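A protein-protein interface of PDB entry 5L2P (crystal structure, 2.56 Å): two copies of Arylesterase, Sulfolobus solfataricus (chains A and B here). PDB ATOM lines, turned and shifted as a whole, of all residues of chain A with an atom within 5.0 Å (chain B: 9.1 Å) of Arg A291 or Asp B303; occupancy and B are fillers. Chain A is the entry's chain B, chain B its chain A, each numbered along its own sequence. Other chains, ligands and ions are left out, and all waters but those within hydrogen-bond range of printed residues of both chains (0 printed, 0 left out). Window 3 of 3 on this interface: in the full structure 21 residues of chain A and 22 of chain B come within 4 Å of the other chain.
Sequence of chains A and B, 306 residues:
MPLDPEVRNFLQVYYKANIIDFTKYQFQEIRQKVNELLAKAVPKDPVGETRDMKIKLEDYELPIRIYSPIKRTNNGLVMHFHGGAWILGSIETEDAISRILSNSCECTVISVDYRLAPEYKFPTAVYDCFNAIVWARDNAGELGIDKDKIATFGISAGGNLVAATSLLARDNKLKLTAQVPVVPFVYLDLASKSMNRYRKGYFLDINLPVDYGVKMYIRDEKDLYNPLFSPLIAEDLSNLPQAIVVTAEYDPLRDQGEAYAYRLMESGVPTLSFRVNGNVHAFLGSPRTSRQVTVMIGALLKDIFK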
ATOM      1  N   ASP A  45      20.816 -16.892   2.858  1.00  0.00           N
ATOM      2  CA  ASP A  45      19.406 -16.563   3.019  1.00  0.00           C
ATOM      3  C   ASP A  45      19.110 -15.289   2.246  1.00  0.00           C
ATOM      4  O   ASP A  45      19.963 -14.423   2.104  1.00  0.00           O
ATOM      5  CB  ASP A  45      19.014 -16.398   4.488  1.00  0.00           C
ATOM      6  CG  ASP A  45      19.040 -17.716   5.263  1.00  0.00           C
ATOM      7  OD1 ASP A  45      19.798 -18.645   4.953  1.00  0.00           O
ATOM      8  OD2 ASP A  45      18.319 -17.826   6.245  1.00  0.00           O
ATOM      9  N   ILE A 100      22.032 -13.605   7.328  1.00  0.00           N
ATOM     10  CA  ILE A 100      21.281 -14.151   8.414  1.00  0.00           C
ATOM     11  C   ILE A 100      21.216 -13.136   9.605  1.00  0.00           C
ATOM     12  O   ILE A 100      20.191 -12.982  10.296  1.00  0.00           O
ATOM     13  CB  ILE A 100      21.875 -15.453   8.902  1.00  0.00           C
ATOM     14  CG1 ILE A 100      21.785 -16.531   7.839  1.00  0.00           C
ATOM     15  CG2 ILE A 100      21.124 -15.915  10.157  1.00  0.00           C
ATOM     16  CD1 ILE A 100      22.805 -17.650   8.086  1.00  0.00           C
ATOM     17  N   PRO A 287      26.617 -26.113   9.315  1.00  0.00           N
ATOM     18  CA  PRO A 287      25.966 -24.909   8.897  1.00  0.00           C
ATOM     19  C   PRO A 287      24.676 -24.629   9.686  1.00  0.00           C
ATOM     20  O   PRO A 287      24.307 -23.475   9.860  1.00  0.00           O
ATOM     21  CB  PRO A 287      25.683 -25.173   7.409  1.00  0.00           C
ATOM     22  CG  PRO A 287      25.882 -26.609   7.173  1.00  0.00           C
ATOM     23  CD  PRO A 287      26.932 -26.965   8.150  1.00  0.00           C
ATOM     24  N   ARG A 288      24.019 -25.675  10.184  1.00  0.00           N
ATOM     25  CA  ARG A 288      22.829 -25.529  10.992  1.00  0.00           C
ATOM     26  C   ARG A 288      23.193 -24.786  12.273  1.00  0.00           C
ATOM     27  O   ARG A 288      22.463 -23.867  12.689  1.00  0.00           O
ATOM     28  CB  ARG A 288      22.204 -26.896  11.332  1.00  0.00           C
ATOM     29  CG  ARG A 288      20.968 -26.799  12.215  1.00  0.00           C
ATOM     30  CD  ARG A 288      20.356 -28.146  12.587  1.00  0.00           C
ATOM     31  NE  ARG A 288      21.304 -29.172  13.043  1.00  0.00           N
ATOM     32  CZ  ARG A 288      21.939 -29.195  14.228  1.00  0.00           C
ATOM     33  NH1 ARG A 288      21.807 -28.199  15.139  1.00  0.00           N
ATOM     34  NH2 ARG A 288      22.749 -30.232  14.509  1.00  0.00           N
ATOM     35  N   THR A 289      24.287 -25.187  12.925  1.00  0.00           N
ATOM     36  CA  THR A 289      24.701 -24.532  14.164  1.00  0.00           C
ATOM     37  C   THR A 289      25.117 -23.101  13.926  1.00  0.00           C
ATOM     38  O   THR A 289      24.797 -22.193  14.706  1.00  0.00           O
ATOM     39  CB  THR A 289      25.861 -25.253  14.830  1.00  0.00           C
ATOM     40  OG1 THR A 289      25.473 -26.584  15.079  1.00  0.00           O
ATOM     41  CG2 THR A 289      26.232 -24.619  16.199  1.00  0.00           C
ATOM     42  N   SER A 290      25.839 -22.897  12.842  1.00  0.00           N
ATOM     43  CA  SER A 290      26.340 -21.560  12.500  1.00  0.00           C
ATOM     44  C   SER A 290      25.157 -20.595  12.306  1.00  0.00           C
ATOM     45  O   SER A 290      25.215 -19.438  12.677  1.00  0.00           O
ATOM     46  CB  SER A 290      27.178 -21.656  11.233  1.00  0.00           C
ATOM     47  OG  SER A 290      27.563 -20.388  10.814  1.00  0.00           O
ATOM     48  N   ARG A 291      24.103 -21.104  11.688  1.00  0.00           N
ATOM     49  CA  ARG A 291      22.911 -20.336  11.448  1.00  0.00           C
ATOM     50  C   ARG A 291      22.181 -20.019  12.762  1.00  0.00           C
ATOM     51  O   ARG A 291      21.837 -18.852  13.005  1.00  0.00           O
ATOM     52  CB  ARG A 291      21.992 -21.095  10.514  1.00  0.00           C
ATOM     53  CG  ARG A 291      20.700 -20.366  10.247  1.00  0.00           C
ATOM     54  CD  ARG A 291      19.977 -20.928   9.025  1.00  0.00           C
ATOM     55  NE  ARG A 291      18.753 -20.193   8.801  1.00  0.00           N
ATOM     56  CZ  ARG A 291      17.643 -20.328   9.540  1.00  0.00           C
ATOM     57  NH1 ARG A 291      17.602 -21.211  10.552  1.00  0.00           N
ATOM     58  NH2 ARG A 291      16.560 -19.588   9.255  1.00  0.00           N
ATOM     59  N   GLN A 292      21.990 -21.043  13.598  1.00  0.00           N
ATOM     60  CA  GLN A 292      21.326 -20.866  14.878  1.00  0.00           C
ATOM     61  C   GLN A 292      22.037 -19.873  15.811  1.00  0.00           C
ATOM     62  O   GLN A 292      21.381 -19.065  16.480  1.00  0.00           O
ATOM     63  CB  GLN A 292      21.120 -22.210  15.560  1.00  0.00           C
ATOM     64  CG  GLN A 292      20.006 -23.004  14.915  1.00  0.00           C
ATOM     65  CD  GLN A 292      19.793 -24.360  15.562  1.00  0.00           C
ATOM     66  OE1 GLN A 292      20.720 -25.134  15.763  1.00  0.00           O
ATOM     67  NE2 GLN A 292      18.561 -24.678  15.829  1.00  0.00           N
ATOM     68  N   VAL A 293      23.365 -19.911  15.809  1.00  0.00           N
ATOM     69  CA  VAL A 293      24.145 -18.956  16.608  1.00  0.00           C
ATOM     70  C   VAL A 293      23.920 -17.526  16.131  1.00  0.00           C
ATOM     71  O   VAL A 293      23.788 -16.602  16.914  1.00  0.00           O
ATOM     72  CB  VAL A 293      25.649 -19.303  16.589  1.00  0.00           C
ATOM     73  CG1 VAL A 293      26.490 -18.196  17.205  1.00  0.00           C
ATOM     74  CG2 VAL A 293      25.875 -20.609  17.341  1.00  0.00           C
ATOM     75  N   THR A 294      23.884 -17.358  14.822  1.00  0.00           N
ATOM     76  CA  THR A 294      23.730 -16.029  14.242  1.00  0.00           C
ATOM     77  C   THR A 294      22.315 -15.478  14.482  1.00  0.00           C
ATOM     78  O   THR A 294      22.129 -14.288  14.663  1.00  0.00           O
ATOM     79  CB  THR A 294      24.048 -16.056  12.738  1.00  0.00           C
ATOM     80  OG1 THR A 294      25.303 -16.725  12.563  1.00  0.00           O
ATOM     81  CG2 THR A 294      24.161 -14.651  12.194  1.00  0.00           C
ATOM     82  N   VAL A 295      21.334 -16.375  14.481  1.00  0.00           N
ATOM     83  CA  VAL A 295      19.971 -16.038  14.780  1.00  0.00           C
ATOM     84  C   VAL A 295      19.832 -15.603  16.237  1.00  0.00           C
ATOM     85  O   VAL A 295      19.145 -14.625  16.530  1.00  0.00           O
ATOM     86  CB  VAL A 295      19.040 -17.214  14.487  1.00  0.00           C
ATOM     87  CG1 VAL A 295      17.649 -16.980  15.101  1.00  0.00           C
ATOM     88  CG2 VAL A 295      18.898 -17.380  12.989  1.00  0.00           C
ATOM     89  N   THR B  73       2.270 -14.805  15.363  1.00  0.00           N
ATOM     90  CA  THR B  73       2.653 -14.931  13.958  1.00  0.00           C
ATOM     91  C   THR B  73       2.858 -16.384  13.504  1.00  0.00           C
ATOM     92  O   THR B  73       3.248 -16.606  12.345  1.00  0.00           O
ATOM     93  CB  THR B  73       3.959 -14.197  13.677  1.00  0.00           C
ATOM     94  OG1 THR B  73       4.984 -14.731  14.527  1.00  0.00           O
ATOM     95  CG2 THR B  73       3.808 -12.732  13.938  1.00  0.00           C
ATOM     96  N   ASN B  74       2.624 -17.361  14.386  1.00  0.00           N
ATOM     97  CA  ASN B  74       2.641 -18.756  13.963  1.00  0.00           C
ATOM     98  C   ASN B  74       1.694 -19.623  14.791  1.00  0.00           C
ATOM     99  O   ASN B  74       1.190 -19.194  15.839  1.00  0.00           O
ATOM    100  CB  ASN B  74       4.061 -19.316  13.986  1.00  0.00           C
ATOM    101  CG  ASN B  74       4.637 -19.377  15.370  1.00  0.00           C
ATOM    102  OD1 ASN B  74       4.273 -20.230  16.175  1.00  0.00           O
ATOM    103  ND2 ASN B  74       5.552 -18.462  15.669  1.00  0.00           N
ATOM    104  N   SER B 104       8.543 -13.933  22.514  1.00  0.00           N
ATOM    105  CA  SER B 104       9.712 -14.193  21.673  1.00  0.00           C
ATOM    106  C   SER B 104       9.376 -15.216  20.598  1.00  0.00           C
ATOM    107  O   SER B 104       9.744 -15.052  19.444  1.00  0.00           O
ATOM    108  CB  SER B 104      10.845 -14.752  22.501  1.00  0.00           C
ATOM    109  OG  SER B 104      11.284 -13.818  23.450  1.00  0.00           O
ATOM    110  N   CYS B 105       8.692 -16.288  21.000  1.00  0.00           N
ATOM    111  CA  CYS B 105       8.202 -17.300  20.062  1.00  0.00           C
ATOM    112  C   CYS B 105       7.111 -16.770  19.143  1.00  0.00           C
ATOM    113  O   CYS B 105       6.941 -17.277  18.033  1.00  0.00           O
ATOM    114  CB  CYS B 105       7.611 -18.489  20.823  1.00  0.00           C
ATOM    115  SG  CYS B 105       8.852 -19.472  21.666  1.00  0.00           S
ATOM    116  N   GLU B 106       6.349 -15.792  19.637  1.00  0.00           N
ATOM    117  CA  GLU B 106       5.171 -15.257  18.967  1.00  0.00           C
ATOM    118  C   GLU B 106       4.155 -16.363  18.755  1.00  0.00           C
ATOM    119  O   GLU B 106       3.555 -16.514  17.667  1.00  0.00           O
ATOM    120  CB  GLU B 106       5.556 -14.561  17.660  1.00  0.00           C
ATOM    121  CG  GLU B 106       6.413 -13.329  17.903  1.00  0.00           C
ATOM    122  CD  GLU B 106       6.983 -12.734  16.625  1.00  0.00           C
ATOM    123  OE1 GLU B 106       6.313 -12.828  15.561  1.00  0.00           O
ATOM    124  OE2 GLU B 106       8.119 -12.191  16.701  1.00  0.00           O
ATOM    125  N   LYS B 149       3.481 -29.015  15.442  1.00  0.00           N
ATOM    126  CA  LYS B 149       4.330 -27.917  15.925  1.00  0.00           C
ATOM    127  C   LYS B 149       4.239 -27.726  17.441  1.00  0.00           C
ATOM    128  O   LYS B 149       4.179 -26.614  17.936  1.00  0.00           O
ATOM    129  CB  LYS B 149       3.997 -26.610  15.222  1.00  0.00           C
ATOM    130  CG  LYS B 149       4.286 -26.580  13.749  1.00  0.00           C
ATOM    131  CD  LYS B 149       3.874 -25.217  13.200  1.00  0.00           C
ATOM    132  CE  LYS B 149       4.008 -25.053  11.700  1.00  0.00           C
ATOM    133  NZ  LYS B 149       5.383 -25.325  11.289  1.00  0.00           N
ATOM    134  N   THR B 177       7.864 -31.470  17.986  1.00  0.00           N
ATOM    135  CA  THR B 177       8.764 -30.855  17.030  1.00  0.00           C
ATOM    136  C   THR B 177      10.103 -30.505  17.653  1.00  0.00           C
ATOM    137  O   THR B 177      11.120 -30.514  16.959  1.00  0.00           O
ATOM    138  CB  THR B 177       8.119 -29.633  16.320  1.00  0.00           C
ATOM    139  OG1 THR B 177       9.001 -29.153  15.302  1.00  0.00           O
ATOM    140  CG2 THR B 177       7.850 -28.509  17.282  1.00  0.00           C
ATOM    141  N   ALA B 178      10.108 -30.199  18.945  1.00  0.00           N
ATOM    142  CA  ALA B 178      11.318 -29.780  19.643  1.00  0.00           C
ATOM    143  C   ALA B 178      11.244 -29.984  21.153  1.00  0.00           C
ATOM    144  O   ALA B 178      10.182 -30.151  21.722  1.00  0.00           O
ATOM    145  CB  ALA B 178      11.596 -28.323  19.354  1.00  0.00           C
ATOM    146  N   GLN B 242      14.302 -32.825  17.993  1.00  0.00           N
ATOM    147  CA  GLN B 242      15.353 -31.831  17.907  1.00  0.00           C
ATOM    148  C   GLN B 242      15.480 -31.054  19.244  1.00  0.00           C
ATOM    149  O   GLN B 242      14.460 -30.529  19.787  1.00  0.00           O
ATOM    150  CB  GLN B 242      14.977 -30.899  16.746  1.00  0.00           C
ATOM    151  CG  GLN B 242      15.915 -29.743  16.488  1.00  0.00           C
ATOM    152  CD  GLN B 242      15.449 -28.891  15.311  1.00  0.00           C
ATOM    153  OE1 GLN B 242      14.321 -29.055  14.814  1.00  0.00           O
ATOM    154  NE2 GLN B 242      16.321 -27.986  14.848  1.00  0.00           N
ATOM    155  N   ILE B 244      17.344 -28.261  22.110  1.00  0.00           N
ATOM    156  CA  ILE B 244      18.161 -27.135  22.514  1.00  0.00           C
ATOM    157  C   ILE B 244      18.454 -27.314  24.003  1.00  0.00           C
ATOM    158  O   ILE B 244      17.607 -27.041  24.830  1.00  0.00           O
ATOM    159  CB  ILE B 244      17.433 -25.804  22.269  1.00  0.00           C
ATOM    160  CG1 ILE B 244      17.135 -25.658  20.780  1.00  0.00           C
ATOM    161  CG2 ILE B 244      18.265 -24.622  22.754  1.00  0.00           C
ATOM    162  CD1 ILE B 244      16.172 -24.548  20.415  1.00  0.00           C
ATOM    163  N   LEU B 272      21.424 -28.382  19.422  1.00  0.00           N
ATOM    164  CA  LEU B 272      22.239 -27.259  19.825  1.00  0.00           C
ATOM    165  C   LEU B 272      22.405 -27.359  21.326  1.00  0.00           C
ATOM    166  O   LEU B 272      21.524 -27.697  22.046  1.00  0.00           O
ATOM    167  CB  LEU B 272      21.583 -25.958  19.413  1.00  0.00           C
ATOM    168  CG  LEU B 272      22.364 -24.703  19.716  1.00  0.00           C
ATOM    169  CD1 LEU B 272      23.554 -24.542  18.786  1.00  0.00           C
ATOM    170  CD2 LEU B 272      21.425 -23.487  19.615  1.00  0.00           C
ATOM    171  N   VAL B 295      14.861 -15.240  25.366  1.00  0.00           N
ATOM    172  CA  VAL B 295      14.705 -14.601  24.057  1.00  0.00           C
ATOM    173  C   VAL B 295      15.445 -15.362  22.941  1.00  0.00           C
ATOM    174  O   VAL B 295      14.902 -15.523  21.845  1.00  0.00           O
ATOM    175  CB  VAL B 295      15.182 -13.130  24.108  1.00  0.00           C
ATOM    176  CG1 VAL B 295      15.389 -12.529  22.738  1.00  0.00           C
ATOM    177  CG2 VAL B 295      14.169 -12.297  24.855  1.00  0.00           C
ATOM    178  N   MET B 296      16.665 -15.803  23.235  1.00  0.00           N
ATOM    179  CA  MET B 296      17.432 -16.651  22.271  1.00  0.00           C
ATOM    180  C   MET B 296      16.672 -17.934  21.905  1.00  0.00           C
ATOM    181  O   MET B 296      16.541 -18.310  20.722  1.00  0.00           O
ATOM    182  CB  MET B 296      18.810 -17.037  22.840  1.00  0.00           C
ATOM    183  CG  MET B 296      19.749 -15.866  22.913  1.00  0.00           C
ATOM    184  SD  MET B 296      21.442 -16.277  23.322  1.00  0.00           S
ATOM    185  CE  MET B 296      21.249 -16.877  24.970  1.00  0.00           C
ATOM    186  N   ILE B 297      16.178 -18.608  22.941  1.00  0.00           N
ATOM    187  CA  ILE B 297      15.440 -19.835  22.750  1.00  0.00           C
ATOM    188  C   ILE B 297      14.206 -19.572  21.918  1.00  0.00           C
ATOM    189  O   ILE B 297      13.891 -20.363  21.041  1.00  0.00           O
ATOM    190  CB  ILE B 297      15.079 -20.466  24.094  1.00  0.00           C
ATOM    191  CG1 ILE B 297      16.325 -21.093  24.744  1.00  0.00           C
ATOM    192  CG2 ILE B 297      13.975 -21.506  23.950  1.00  0.00           C
ATOM    193  CD1 ILE B 297      16.146 -21.456  26.227  1.00  0.00           C
ATOM    194  N   GLY B 298      13.480 -18.487  22.219  1.00  0.00           N
ATOM    195  CA  GLY B 298      12.277 -18.113  21.470  1.00  0.00           C
ATOM    196  C   GLY B 298      12.540 -17.879  19.989  1.00  0.00           C
ATOM    197  O   GLY B 298      11.766 -18.310  19.138  1.00  0.00           O
ATOM    198  N   ALA B 299      13.635 -17.196  19.691  1.00  0.00           N
ATOM    199  CA  ALA B 299      14.039 -16.960  18.311  1.00  0.00           C
ATOM    200  C   ALA B 299      14.276 -18.279  17.533  1.00  0.00           C
ATOM    201  O   ALA B 299      13.912 -18.389  16.369  1.00  0.00           O
ATOM    202  CB  ALA B 299      15.299 -16.108  18.264  1.00  0.00           C
ATOM    203  N   LEU B 300      14.883 -19.258  18.189  1.00  0.00           N
ATOM    204  CA  LEU B 300      15.122 -20.562  17.589  1.00  0.00           C
ATOM    205  C   LEU B 300      13.867 -21.370  17.418  1.00  0.00           C
ATOM    206  O   LEU B 300      13.676 -21.989  16.383  1.00  0.00           O
ATOM    207  CB  LEU B 300      16.129 -21.364  18.419  1.00  0.00           C
ATOM    208  CG  LEU B 300      17.550 -20.779  18.428  1.00  0.00           C
ATOM    209  CD1 LEU B 300      18.410 -21.578  19.402  1.00  0.00           C
ATOM    210  CD2 LEU B 300      18.148 -20.780  17.028  1.00  0.00           C
ATOM    211  N   LEU B 301      12.999 -21.369  18.426  1.00  0.00           N
ATOM    212  CA  LEU B 301      11.676 -22.024  18.303  1.00  0.00           C
ATOM    213  C   LEU B 301      10.809 -21.404  17.226  1.00  0.00           C
ATOM    214  O   LEU B 301      10.172 -22.108  16.430  1.00  0.00           O
ATOM    215  CB  LEU B 301      10.929 -21.991  19.615  1.00  0.00           C
ATOM    216  CG  LEU B 301      11.514 -22.891  20.714  1.00  0.00           C
ATOM    217  CD1 LEU B 301      10.776 -22.629  22.006  1.00  0.00           C
ATOM    218  CD2 LEU B 301      11.415 -24.383  20.352  1.00  0.00           C
ATOM    219  N   LYS B 302      10.788 -20.082  17.207  1.00  0.00           N
ATOM    220  CA  LYS B 302      10.057 -19.335  16.166  1.00  0.00           C
ATOM    221  C   LYS B 302      10.544 -19.759  14.780  1.00  0.00           C
ATOM    222  O   LYS B 302       9.775 -19.949  13.869  1.00  0.00           O
ATOM    223  CB  LYS B 302      10.289 -17.851  16.373  1.00  0.00           C
ATOM    224  CG  LYS B 302       9.674 -16.958  15.324  1.00  0.00           C
ATOM    225  CD  LYS B 302      10.098 -15.533  15.598  1.00  0.00           C
ATOM    226  CE  LYS B 302       9.732 -14.603  14.473  1.00  0.00           C
ATOM    227  NZ  LYS B 302      10.162 -13.218  14.802  1.00  0.00           N
ATOM    228  N   ASP B 303      11.844 -19.938  14.652  1.00  0.00           N
ATOM    229  CA  ASP B 303      12.448 -20.394  13.414  1.00  0.00           C
ATOM    230  C   ASP B 303      12.092 -21.826  13.055  1.00  0.00           C
ATOM    231  O   ASP B 303      11.914 -22.144  11.898  1.00  0.00           O
ATOM    232  CB  ASP B 303      13.964 -20.264  13.515  1.00  0.00           C
ATOM    233  CG  ASP B 303      14.591 -20.173  12.232  1.00  0.00           C
ATOM    234  OD1 ASP B 303      14.687 -21.238  11.617  1.00  0.00           O
ATOM    235  OD2 ASP B 303      14.963 -19.050  11.854  1.00  0.00           O
ATOM    236  N   ILE B 304      11.989 -22.693  14.042  1.00  0.00           N
ATOM    237  CA  ILE B 304      11.482 -24.046  13.793  1.00  0.00           C
ATOM    238  C   ILE B 304       9.990 -24.047  13.436  1.00  0.00           C
ATOM    239  O   ILE B 304       9.557 -24.855  12.651  1.00  0.00           O
ATOM    240  CB  ILE B 304      11.712 -24.931  15.033  1.00  0.00           C
ATOM    241  CG1 ILE B 304      13.200 -25.207  15.221  1.00  0.00           C
ATOM    242  CG2 ILE B 304      10.954 -26.250  14.929  1.00  0.00           C
ATOM    243  CD1 ILE B 304      13.567 -25.679  16.608  1.00  0.00           C
ATOM    244  N   PHE B 305       9.197 -23.158  14.030  1.00  0.00           N
ATOM    245  CA  PHE B 305       7.764 -23.059  13.741  1.00  0.00           C
ATOM    246  C   PHE B 305       7.438 -22.464  12.387  1.00  0.00           C
ATOM    247  O   PHE B 305       6.419 -22.843  11.808  1.00  0.00           O
ATOM    248  CB  PHE B 305       7.003 -22.285  14.834  1.00  0.00           C
ATOM    249  CG  PHE B 305       6.986 -22.968  16.173  1.00  0.00           C
ATOM    250  CD1 PHE B 305       6.848 -24.349  16.278  1.00  0.00           C
ATOM    251  CD2 PHE B 305       7.089 -22.225  17.329  1.00  0.00           C
ATOM    252  CE1 PHE B 305       6.832 -24.977  17.515  1.00  0.00           C
ATOM    253  CE2 PHE B 305       7.084 -22.832  18.573  1.00  0.00           C
ATOM    254  CZ  PHE B 305       6.949 -24.213  18.673  1.00  0.00           C
ATOM    255  N   LYS B 306       8.260 -21.571  11.845  1.00  0.00           N
ATOM    256  CA  LYS B 306       8.183 -21.249  10.364  1.00  0.00           C
ATOM    257  C   LYS B 306       7.904 -22.502   9.499  1.00  0.00           C
ATOM    258  O   LYS B 306       7.156 -22.459   8.514  1.00  0.00           O
ATOM    259  CB  LYS B 306       9.493 -20.613   9.865  1.00  0.00           C
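The side-chain carboxylate (OD2) of Asp B303 lies within salt-bridge range of the guanidinium group (NH2) of Arg A291, 3.1 Å away.
The guanidinium group (NE) of Arg A291 is in salt-bridge range of the side-chain carboxylate (OD2) of Asp A45 (3.5 Å). OE1 of Gln A292 lies within hydrogen-bond range of NH1 of Arg A288.
Leu B272 touches Thr A289. OE1 of Gln A292 touches CB of Leu B272, 3.8 Å away. CG of Gln A292 touches CD2 of Leu B300 (3.6 Å).
Arg A291 touches just one residue of chain B: Asp B303 (3.1 Å). Asp B303 touches just one residue of chain A: Arg A291 (3.1 Å). No residue of chain B comes within 4 Å of Ser A290. No residue of chain B comes within 4 Å of Thr A294. Printed residues of chain A within 4 Å of Leu B300: Gln A292 (3.6 Å). Of the printed residues of chain B, Thr A289 touches Leu B272 (3.7 Å). Ile A100 touches none of the printed residues of chain B. Thr B73 touches none of the printed residues of chain A. The nearest residue of chain A that does not touch Asp B303 is Val A295 (4.4 Å). The nearest printed residue of chain B that does not touch Thr A289 is Leu B300 (7.2 Å).
Printed residues of chain B that touch a printed residue of chain A: Leu B272, Leu B300 and Asp B303. Of the 11 printed residues of chain A, 3 touch a printed residue of chain B. Along chain A the printed residues that touch a printed residue of chain B span positions 289 to 292. Among the printed residues, 4 pairs touch across the chains. Among the printed residues, Asp or Glu carboxylates within 4 Å of a Lys or Arg side-chain nitrogen of the other chain: Arg A291 with Asp B303.
1 position is printed for both chains. Of the 4 pairs that touch across the chains among the printed residues, none has its exchanged pair printed and touching as well.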
